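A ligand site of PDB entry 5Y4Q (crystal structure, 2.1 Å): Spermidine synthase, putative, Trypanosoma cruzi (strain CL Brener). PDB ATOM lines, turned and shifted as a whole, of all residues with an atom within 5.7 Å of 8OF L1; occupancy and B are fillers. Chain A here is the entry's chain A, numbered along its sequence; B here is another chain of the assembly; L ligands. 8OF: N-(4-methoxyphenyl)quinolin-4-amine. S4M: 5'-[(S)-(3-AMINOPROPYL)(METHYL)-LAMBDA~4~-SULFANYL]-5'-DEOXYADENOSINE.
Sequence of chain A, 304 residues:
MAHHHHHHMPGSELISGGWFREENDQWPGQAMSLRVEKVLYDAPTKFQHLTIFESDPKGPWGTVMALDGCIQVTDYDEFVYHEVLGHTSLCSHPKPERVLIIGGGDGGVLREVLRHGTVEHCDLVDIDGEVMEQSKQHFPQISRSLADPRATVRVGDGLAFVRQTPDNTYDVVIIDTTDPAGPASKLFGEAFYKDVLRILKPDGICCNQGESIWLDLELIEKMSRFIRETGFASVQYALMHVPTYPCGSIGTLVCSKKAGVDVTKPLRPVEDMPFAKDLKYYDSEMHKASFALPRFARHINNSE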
ATOM      1  N   GLU A  22      -7.991   1.854 -19.206  1.00  0.00           N
ATOM      2  CA  GLU A  22      -6.775   1.665 -18.451  1.00  0.00           C
ATOM      3  C   GLU A  22      -5.624   2.187 -19.258  1.00  0.00           C
ATOM      4  O   GLU A  22      -5.425   1.789 -20.421  1.00  0.00           O
ATOM      5  CB  GLU A  22      -6.608   0.166 -18.232  1.00  0.00           C
ATOM      6  CG  GLU A  22      -5.655  -0.274 -17.132  1.00  0.00           C
ATOM      7  CD  GLU A  22      -5.669  -1.784 -16.993  1.00  0.00           C
ATOM      8  OE1 GLU A  22      -6.065  -2.468 -17.953  1.00  0.00           O
ATOM      9  OE2 GLU A  22      -5.267  -2.286 -15.927  1.00  0.00           O
ATOM     10  N   MET A  32      -6.157   0.474 -23.014  1.00  0.00           N
ATOM     11  CA  MET A  32      -6.928  -0.743 -23.078  1.00  0.00           C
ATOM     12  C   MET A  32      -8.280  -0.434 -22.428  1.00  0.00           C
ATOM     13  O   MET A  32      -8.324   0.136 -21.325  1.00  0.00           O
ATOM     14  CB  MET A  32      -6.191  -1.832 -22.281  1.00  0.00           C
ATOM     15  CG  MET A  32      -6.150  -3.224 -22.908  1.00  0.00           C
ATOM     16  SD  MET A  32      -7.654  -3.861 -23.660  1.00  0.00           S
ATOM     17  CE  MET A  32      -8.688  -4.075 -22.201  1.00  0.00           C
ATOM     18  N   LEU A  34     -12.403  -1.786 -21.459  1.00  0.00           N
ATOM     19  CA  LEU A  34     -13.481  -2.763 -21.347  1.00  0.00           C
ATOM     20  C   LEU A  34     -14.825  -2.086 -21.156  1.00  0.00           C
ATOM     21  O   LEU A  34     -14.951  -1.191 -20.343  1.00  0.00           O
ATOM     22  CB  LEU A  34     -13.234  -3.724 -20.175  1.00  0.00           C
ATOM     23  CG  LEU A  34     -12.079  -4.721 -20.245  1.00  0.00           C
ATOM     24  CD1 LEU A  34     -11.966  -5.441 -18.910  1.00  0.00           C
ATOM     25  CD2 LEU A  34     -12.265  -5.728 -21.377  1.00  0.00           C
ATOM     26  N   TRP A  61     -14.485 -11.944 -20.062  1.00  0.00           N
ATOM     27  CA  TRP A  61     -13.824 -11.500 -18.791  1.00  0.00           C
ATOM     28  C   TRP A  61     -14.584 -11.735 -17.463  1.00  0.00           C
ATOM     29  O   TRP A  61     -13.946 -12.003 -16.417  1.00  0.00           O
ATOM     30  CB  TRP A  61     -13.348 -10.062 -18.900  1.00  0.00           C
ATOM     31  CG  TRP A  61     -12.439  -9.922 -20.050  1.00  0.00           C
ATOM     32  CD1 TRP A  61     -12.757  -9.403 -21.276  1.00  0.00           C
ATOM     33  CD2 TRP A  61     -11.068 -10.370 -20.125  1.00  0.00           C
ATOM     34  NE1 TRP A  61     -11.641  -9.477 -22.096  1.00  0.00           N
ATOM     35  CE2 TRP A  61     -10.600 -10.061 -21.423  1.00  0.00           C
ATOM     36  CE3 TRP A  61     -10.175 -10.986 -19.208  1.00  0.00           C
ATOM     37  CZ2 TRP A  61      -9.283 -10.360 -21.850  1.00  0.00           C
ATOM     38  CZ3 TRP A  61      -8.855 -11.301 -19.637  1.00  0.00           C
ATOM     39  CH2 TRP A  61      -8.444 -10.986 -20.949  1.00  0.00           C
ATOM     40  N   CYS A  70      -6.053   0.186 -12.241  1.00  0.00           N
ATOM     41  CA  CYS A  70      -5.346  -0.931 -12.855  1.00  0.00           C
ATOM     42  C   CYS A  70      -6.087  -2.203 -12.512  1.00  0.00           C
ATOM     43  O   CYS A  70      -6.270  -2.534 -11.336  1.00  0.00           O
ATOM     44  CB  CYS A  70      -3.880  -1.020 -12.364  1.00  0.00           C
ATOM     45  SG  CYS A  70      -2.852   0.448 -12.698  1.00  0.00           S
ATOM     46  N   ILE A  71      -6.470  -2.945 -13.546  1.00  0.00           N
ATOM     47  CA  ILE A  71      -7.119  -4.258 -13.364  1.00  0.00           C
ATOM     48  C   ILE A  71      -6.180  -5.220 -12.645  1.00  0.00           C
ATOM     49  O   ILE A  71      -5.007  -5.333 -13.026  1.00  0.00           O
ATOM     50  CB  ILE A  71      -7.628  -4.836 -14.707  1.00  0.00           C
ATOM     51  CG1 ILE A  71      -8.798  -3.962 -15.229  1.00  0.00           C
ATOM     52  CG2 ILE A  71      -8.059  -6.298 -14.553  1.00  0.00           C
ATOM     53  CD1 ILE A  71      -8.992  -3.934 -16.733  1.00  0.00           C
ATOM     54  N   GLN A  72      -6.706  -5.908 -11.633  1.00  0.00           N
ATOM     55  CA  GLN A  72      -5.925  -6.825 -10.808  1.00  0.00           C
ATOM     56  C   GLN A  72      -6.449  -8.247 -10.850  1.00  0.00           C
ATOM     57  O   GLN A  72      -5.701  -9.188 -10.618  1.00  0.00           O
ATOM     58  CB  GLN A  72      -5.827  -6.337  -9.340  1.00  0.00           C
ATOM     59  CG  GLN A  72      -4.911  -5.114  -9.101  1.00  0.00           C
ATOM     60  CD  GLN A  72      -3.499  -5.217  -9.698  1.00  0.00           C
ATOM     61  OE1 GLN A  72      -2.906  -6.284  -9.791  1.00  0.00           O
ATOM     62  NE2 GLN A  72      -2.959  -4.069 -10.102  1.00  0.00           N
ATOM     63  N   VAL A  73      -7.751  -8.390 -11.138  1.00  0.00           N
ATOM     64  CA  VAL A  73      -8.411  -9.682 -11.104  1.00  0.00           C
ATOM     65  C   VAL A  73      -9.552  -9.647 -12.105  1.00  0.00           C
ATOM     66  O   VAL A  73     -10.287  -8.639 -12.180  1.00  0.00           O
ATOM     67  CB  VAL A  73      -9.015 -10.031  -9.702  1.00  0.00           C
ATOM     68  CG1 VAL A  73      -9.598 -11.429  -9.726  1.00  0.00           C
ATOM     69  CG2 VAL A  73      -7.957  -9.984  -8.620  1.00  0.00           C
ATOM     70  N   THR A  74      -9.668 -10.725 -12.889  1.00  0.00           N
ATOM     71  CA  THR A  74     -10.890 -10.995 -13.685  1.00  0.00           C
ATOM     72  C   THR A  74     -11.181 -12.443 -13.460  1.00  0.00           C
ATOM     73  O   THR A  74     -10.251 -13.192 -13.167  1.00  0.00           O
ATOM     74  CB  THR A  74     -10.752 -10.732 -15.206  1.00  0.00           C
ATOM     75  OG1 THR A  74     -10.006 -11.789 -15.835  1.00  0.00           O
ATOM     76  CG2 THR A  74     -10.115  -9.417 -15.494  1.00  0.00           C
ATOM     77  N   ASP A  77      -9.121 -14.825 -16.325  1.00  0.00           N
ATOM     78  CA  ASP A  77      -7.665 -15.092 -16.322  1.00  0.00           C
ATOM     79  C   ASP A  77      -7.020 -15.334 -14.957  1.00  0.00           C
ATOM     80  O   ASP A  77      -5.821 -15.633 -14.881  1.00  0.00           O
ATOM     81  CB  ASP A  77      -6.874 -13.988 -17.083  1.00  0.00           C
ATOM     82  CG  ASP A  77      -7.018 -12.573 -16.464  1.00  0.00           C
ATOM     83  OD1 ASP A  77      -7.560 -12.365 -15.353  1.00  0.00           O
ATOM     84  OD2 ASP A  77      -6.538 -11.613 -17.120  1.00  0.00           O
ATOM     85  N   TYR A  81      -2.151 -16.171 -12.895  1.00  0.00           N
ATOM     86  CA  TYR A  81      -1.222 -15.576 -11.934  1.00  0.00           C
ATOM     87  C   TYR A  81      -1.325 -16.279 -10.595  1.00  0.00           C
ATOM     88  O   TYR A  81      -0.308 -16.470  -9.931  1.00  0.00           O
ATOM     89  CB  TYR A  81      -1.391 -14.048 -11.755  1.00  0.00           C
ATOM     90  CG  TYR A  81      -2.771 -13.477 -12.076  1.00  0.00           C
ATOM     91  CD1 TYR A  81      -3.182 -13.273 -13.414  1.00  0.00           C
ATOM     92  CD2 TYR A  81      -3.673 -13.119 -11.035  1.00  0.00           C
ATOM     93  CE1 TYR A  81      -4.428 -12.754 -13.708  1.00  0.00           C
ATOM     94  CE2 TYR A  81      -4.918 -12.589 -11.320  1.00  0.00           C
ATOM     95  CZ  TYR A  81      -5.296 -12.393 -12.651  1.00  0.00           C
ATOM     96  OH  TYR A  81      -6.524 -11.859 -12.952  1.00  0.00           O
ATOM     97  N   ASP A 176       2.006 -10.727  -3.165  1.00  0.00           N
ATOM     98  CA  ASP A 176       1.009 -10.607  -4.215  1.00  0.00           C
ATOM     99  C   ASP A 176       0.405  -9.202  -4.146  1.00  0.00           C
ATOM    100  O   ASP A 176      -0.746  -9.035  -3.795  1.00  0.00           O
ATOM    101  CB  ASP A 176      -0.038 -11.723  -4.046  1.00  0.00           C
ATOM    102  CG  ASP A 176      -1.115 -11.692  -5.119  1.00  0.00           C
ATOM    103  OD1 ASP A 176      -0.833 -11.283  -6.263  1.00  0.00           O
ATOM    104  OD2 ASP A 176      -2.258 -12.113  -4.805  1.00  0.00           O
ATOM    105  N   THR A 177       1.190  -8.194  -4.495  1.00  0.00           N
ATOM    106  CA  THR A 177       0.761  -6.809  -4.301  1.00  0.00           C
ATOM    107  C   THR A 177       0.501  -6.074  -5.621  1.00  0.00           C
ATOM    108  O   THR A 177       0.505  -6.677  -6.695  1.00  0.00           O
ATOM    109  CB  THR A 177       1.756  -6.017  -3.413  1.00  0.00           C
ATOM    110  OG1 THR A 177       3.049  -6.046  -4.020  1.00  0.00           O
ATOM    111  CG2 THR A 177       1.816  -6.622  -2.034  1.00  0.00           C
ATOM    112  N   GLN A 209       5.073 -10.674  -7.250  1.00  0.00           N
ATOM    113  CA  GLN A 209       4.533 -10.173  -8.517  1.00  0.00           C
ATOM    114  C   GLN A 209       5.659  -9.341  -9.125  1.00  0.00           C
ATOM    115  O   GLN A 209       6.024  -8.285  -8.575  1.00  0.00           O
ATOM    116  CB  GLN A 209       3.276  -9.340  -8.229  1.00  0.00           C
ATOM    117  CG  GLN A 209       2.479  -8.825  -9.422  1.00  0.00           C
ATOM    118  CD  GLN A 209       2.798  -7.380  -9.803  1.00  0.00           C
ATOM    119  OE1 GLN A 209       2.193  -6.442  -9.283  1.00  0.00           O
ATOM    120  NE2 GLN A 209       3.771  -7.198 -10.697  1.00  0.00           N
ATOM    121  N   VAL A 242      -0.482 -14.518 -20.153  1.00  0.00           N
ATOM    122  CA  VAL A 242      -1.773 -13.982 -19.757  1.00  0.00           C
ATOM    123  C   VAL A 242      -2.544 -13.601 -21.056  1.00  0.00           C
ATOM    124  O   VAL A 242      -1.907 -13.248 -22.055  1.00  0.00           O
ATOM    125  CB  VAL A 242      -1.559 -12.851 -18.721  1.00  0.00           C
ATOM    126  CG1 VAL A 242      -2.841 -12.121 -18.392  1.00  0.00           C
ATOM    127  CG2 VAL A 242      -1.035 -13.429 -17.421  1.00  0.00           C
ATOM    128  N   THR A 244      -4.385 -10.951 -21.735  1.00  0.00           N
ATOM    129  CA  THR A 244      -4.062  -9.524 -21.992  1.00  0.00           C
ATOM    130  C   THR A 244      -3.295  -8.861 -20.832  1.00  0.00           C
ATOM    131  O   THR A 244      -3.633  -9.054 -19.649  1.00  0.00           O
ATOM    132  CB  THR A 244      -5.341  -8.700 -22.388  1.00  0.00           C
ATOM    133  OG1 THR A 244      -5.913  -9.204 -23.608  1.00  0.00           O
ATOM    134  CG2 THR A 244      -5.013  -7.199 -22.578  1.00  0.00           C
ATOM    135  N   TYR A 245      -2.265  -8.069 -21.168  1.00  0.00           N
ATOM    136  CA  TYR A 245      -1.542  -7.250 -20.200  1.00  0.00           C
ATOM    137  C   TYR A 245      -0.928  -5.974 -20.844  1.00  0.00           C
ATOM    138  O   TYR A 245       0.235  -5.986 -21.283  1.00  0.00           O
ATOM    139  CB  TYR A 245      -0.509  -8.099 -19.443  1.00  0.00           C
ATOM    140  CG  TYR A 245      -0.127  -7.565 -18.076  1.00  0.00           C
ATOM    141  CD1 TYR A 245      -0.984  -7.681 -16.968  1.00  0.00           C
ATOM    142  CD2 TYR A 245       1.117  -6.952 -17.882  1.00  0.00           C
ATOM    143  CE1 TYR A 245      -0.613  -7.191 -15.708  1.00  0.00           C
ATOM    144  CE2 TYR A 245       1.501  -6.470 -16.635  1.00  0.00           C
ATOM    145  CZ  TYR A 245       0.644  -6.588 -15.557  1.00  0.00           C
ATOM    146  OH  TYR A 245       1.058  -6.099 -14.330  1.00  0.00           O
ATOM    147  N   PRO A 246      -1.707  -4.861 -20.875  1.00  0.00           N
ATOM    148  CA  PRO A 246      -1.370  -3.597 -21.574  1.00  0.00           C
ATOM    149  C   PRO A 246      -0.070  -3.011 -21.057  1.00  0.00           C
ATOM    150  O   PRO A 246       0.577  -2.208 -21.741  1.00  0.00           O
ATOM    151  CB  PRO A 246      -2.544  -2.659 -21.238  1.00  0.00           C
ATOM    152  CG  PRO A 246      -3.571  -3.495 -20.558  1.00  0.00           C
ATOM    153  CD  PRO A 246      -2.880  -4.692 -19.987  1.00  0.00           C
ATOM    154  N   CYS A 247       0.305  -3.424 -19.856  1.00  0.00           N
ATOM    155  CA  CYS A 247       1.543  -3.045 -19.193  1.00  0.00           C
ATOM    156  C   CYS A 247       2.796  -3.872 -19.644  1.00  0.00           C
ATOM    157  O   CYS A 247       3.901  -3.656 -19.150  1.00  0.00           O
ATOM    158  CB  CYS A 247       1.323  -3.059 -17.678  1.00  0.00           C
ATOM    159  SG  CYS A 247      -0.352  -3.628 -17.230  1.00  0.00           S
ATOM    160  N   ILE A 250       3.613 -10.096 -17.458  1.00  0.00           N
ATOM    161  CA  ILE A 250       3.687 -10.232 -16.005  1.00  0.00           C
ATOM    162  C   ILE A 250       4.572 -11.405 -15.674  1.00  0.00           C
ATOM    163  O   ILE A 250       4.525 -12.436 -16.357  1.00  0.00           O
ATOM    164  CB  ILE A 250       2.292 -10.259 -15.309  1.00  0.00           C
ATOM    165  CG1 ILE A 250       2.411 -10.259 -13.789  1.00  0.00           C
ATOM    166  CG2 ILE A 250       1.432 -11.426 -15.760  1.00  0.00           C
ATOM    167  CD1 ILE A 250       2.506  -8.870 -13.177  1.00  0.00           C
ATOM    168  N   GLN B  30     -14.123  -5.209 -25.710  1.00  0.00           N
ATOM    169  CA  GLN B  30     -12.716  -4.911 -25.463  1.00  0.00           C
ATOM    170  C   GLN B  30     -12.168  -4.109 -26.634  1.00  0.00           C
ATOM    171  O   GLN B  30     -12.488  -4.379 -27.781  1.00  0.00           O
ATOM    172  CB  GLN B  30     -11.911  -6.208 -25.242  1.00  0.00           C
ATOM    173  CG  GLN B  30     -10.397  -6.015 -25.022  1.00  0.00           C
ATOM    174  CD  GLN B  30      -9.690  -7.293 -24.616  1.00  0.00           C
ATOM    175  OE1 GLN B  30      -8.490  -7.286 -24.298  1.00  0.00           O
ATOM    176  NE2 GLN B  30     -10.431  -8.404 -24.609  1.00  0.00           N
HETATM  177  C9  8OF L   1      -8.010  -8.137 -19.260  1.00  0.00           C
HETATM  178  C12 8OF L   1      -8.219  -6.848 -19.699  1.00  0.00           C
HETATM  179  C4  8OF L   1      -7.021  -8.452 -18.343  1.00  0.00           C
HETATM  180  C8  8OF L   1      -7.417  -5.853 -19.213  1.00  0.00           C
HETATM  181  C13 8OF L   1      -3.093 -10.122 -15.377  1.00  0.00           C
HETATM  182  C14 8OF L   1      -3.979  -8.426 -13.926  1.00  0.00           C
HETATM  183  C15 8OF L   1      -2.243 -10.553 -14.385  1.00  0.00           C
HETATM  184  C16 8OF L   1      -3.153  -8.888 -12.909  1.00  0.00           C
HETATM  185  C6  8OF L   1      -4.441  -6.538 -16.527  1.00  0.00           C
HETATM  186  C11 8OF L   1      -4.719  -5.293 -17.008  1.00  0.00           C
HETATM  187  C1  8OF L   1      -6.218  -7.446 -17.848  1.00  0.00           C
HETATM  188  C3  8OF L   1      -6.425  -6.137 -18.298  1.00  0.00           C
HETATM  189  C10 8OF L   1      -3.913  -9.031 -15.170  1.00  0.00           C
HETATM  190  C2  8OF L   1      -5.203  -7.624 -16.914  1.00  0.00           C
HETATM  191  C17 8OF L   1      -2.279  -9.951 -13.141  1.00  0.00           C
HETATM  192  C19 8OF L   1      -1.367  -9.792 -10.970  1.00  0.00           C
HETATM  193  N7  8OF L   1      -5.700  -5.101 -17.885  1.00  0.00           N
HETATM  194  N5  8OF L   1      -4.629  -8.716 -16.325  1.00  0.00           N
HETATM  195  O18 8OF L   1      -1.406 -10.517 -12.212  1.00  0.00           O
HETATM  196  CA  S4M L   2      -4.162 -10.166  -7.792  1.00  0.00           C
HETATM  197  N   S4M L   2      -4.203 -11.247  -6.787  1.00  0.00           N
HETATM  198  CB  S4M L   2      -2.982  -9.291  -7.471  1.00  0.00           C
HETATM  199  CG  S4M L   2      -3.364  -8.023  -6.749  1.00  0.00           C
HETATM  200  SD  S4M L   2      -3.767  -8.307  -4.999  1.00  0.00           S
HETATM  201  CE  S4M L   2      -5.472  -7.697  -5.207  1.00  0.00           C
HETATM  202  C5' S4M L   2      -3.005  -6.741  -4.435  1.00  0.00           C
HETATM  203  C4' S4M L   2      -3.212  -6.519  -2.949  1.00  0.00           C
HETATM  204  O4' S4M L   2      -2.045  -5.997  -2.323  1.00  0.00           O
HETATM  205  C1' S4M L   2      -2.542  -5.169  -1.267  1.00  0.00           C
HETATM  206  C2' S4M L   2      -3.690  -4.421  -1.872  1.00  0.00           C
HETATM  207  O2' S4M L   2      -4.597  -3.993  -0.865  1.00  0.00           O
HETATM  208  C3' S4M L   2      -4.275  -5.484  -2.781  1.00  0.00           C
HETATM  209  O3' S4M L   2      -5.409  -6.128  -2.222  1.00  0.00           O
HETATM  210  N9  S4M L   2      -1.470  -4.331  -0.751  1.00  0.00           N
HETATM  211  C8  S4M L   2      -0.872  -3.245  -1.322  1.00  0.00           C
HETATM  212  N7  S4M L   2       0.074  -2.757  -0.540  1.00  0.00           N
HETATM  213  C5  S4M L   2       0.088  -3.558   0.575  1.00  0.00           C
HETATM  214  C6  S4M L   2       0.853  -3.538   1.737  1.00  0.00           C
HETATM  215  N6  S4M L   2       1.858  -2.586   1.973  1.00  0.00           N
HETATM  216  C4  S4M L   2      -0.875  -4.551   0.455  1.00  0.00           C
HETATM  217  N3  S4M L   2      -1.157  -5.512   1.343  1.00  0.00           N
HETATM  218  C2  S4M L   2      -0.354  -5.389   2.400  1.00  0.00           C
HETATM  219  N1  S4M L   2       0.605  -4.486   2.651  1.00  0.00           N
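OD2 of Asp 176 is in salt-bridge range of N of S4M L2. The backbone carbonyl oxygen (O) of Thr 244 lies close to a nitrogen (N5) of 8OF L1, at 3.5 Å. A nitrogen (N7) of 8OF L1 lies within hydrogen-bond range of the side-chain carboxylate (OE1) of Glu 22 (2.7 Å). SD of S4M L2 lies close to O of Asp 176 (3.3 Å).
The side-chain carboxylate (OD1) of Asp 77 lies within hydrogen-bond range of the side-chain hydroxyl (OG1) of Thr 74 (2.6 Å). The indole nitrogen (NE1) of Trp 61 lies close to the side-chain amide nitrogen (NE2) of Gln 30 of chain B (3.0 Å). The backbone carbonyl oxygen (O) of Met 32 sits at hydrogen-bond distance from the backbone NH (N) of Glu 22, at 2.7 Å. The backbone NH (N) of Ile 71 sits at hydrogen-bond distance from the side-chain carboxylate (OE2) of Glu 22, 2.7 Å away. The side-chain hydroxyl (OH) of Tyr 81 sits at hydrogen-bond distance from the backbone NH (N) of Thr 74, 3.3 Å away. OG1 of Thr 244 is in hydrogen-bond range of OE1 of Gln 30 of chain B (3.3 Å). The side-chain hydroxyl of Tyr 81 is in hydrogen-bond range of the side-chain carboxylate of Asp 77, 2.7 Å away. SD of Met 32 sits close to OE1 of Gln 30 of chain B, 3.6 Å away.
Met 32 touches 8OF L1 (CE to C8, 3.7 Å). Trp 61 touches 8OF L1. Ile 71 touches 8OF L1 (O to C14, 3.4 Å). O of Gln 72 touches C16 of 8OF L1, at 3.4 Å. Asp 77 touches 8OF L1. CD1 of Tyr 81 touches C15 of 8OF L1, 3.0 Å away. Val 242 touches 8OF L1 (CG1 to C13, 3.6 Å). Tyr 245 touches 8OF L1. Pro 246 touches 8OF L1 (CD to N7, 3.5 Å). Hydrophobic or aromatic side chains that line 8OF L1: Met 32, Trp 61, Ile 71, Tyr 81, Val 242, Tyr 245 and Pro 246. 11 residues have an atom within 4 Å of 8OF L1: Glu 22, Met 32, Trp 61, Ile 71, Gln 72, Asp 77, Tyr 81, Val 242, Thr 244, Tyr 245 and Pro 246.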
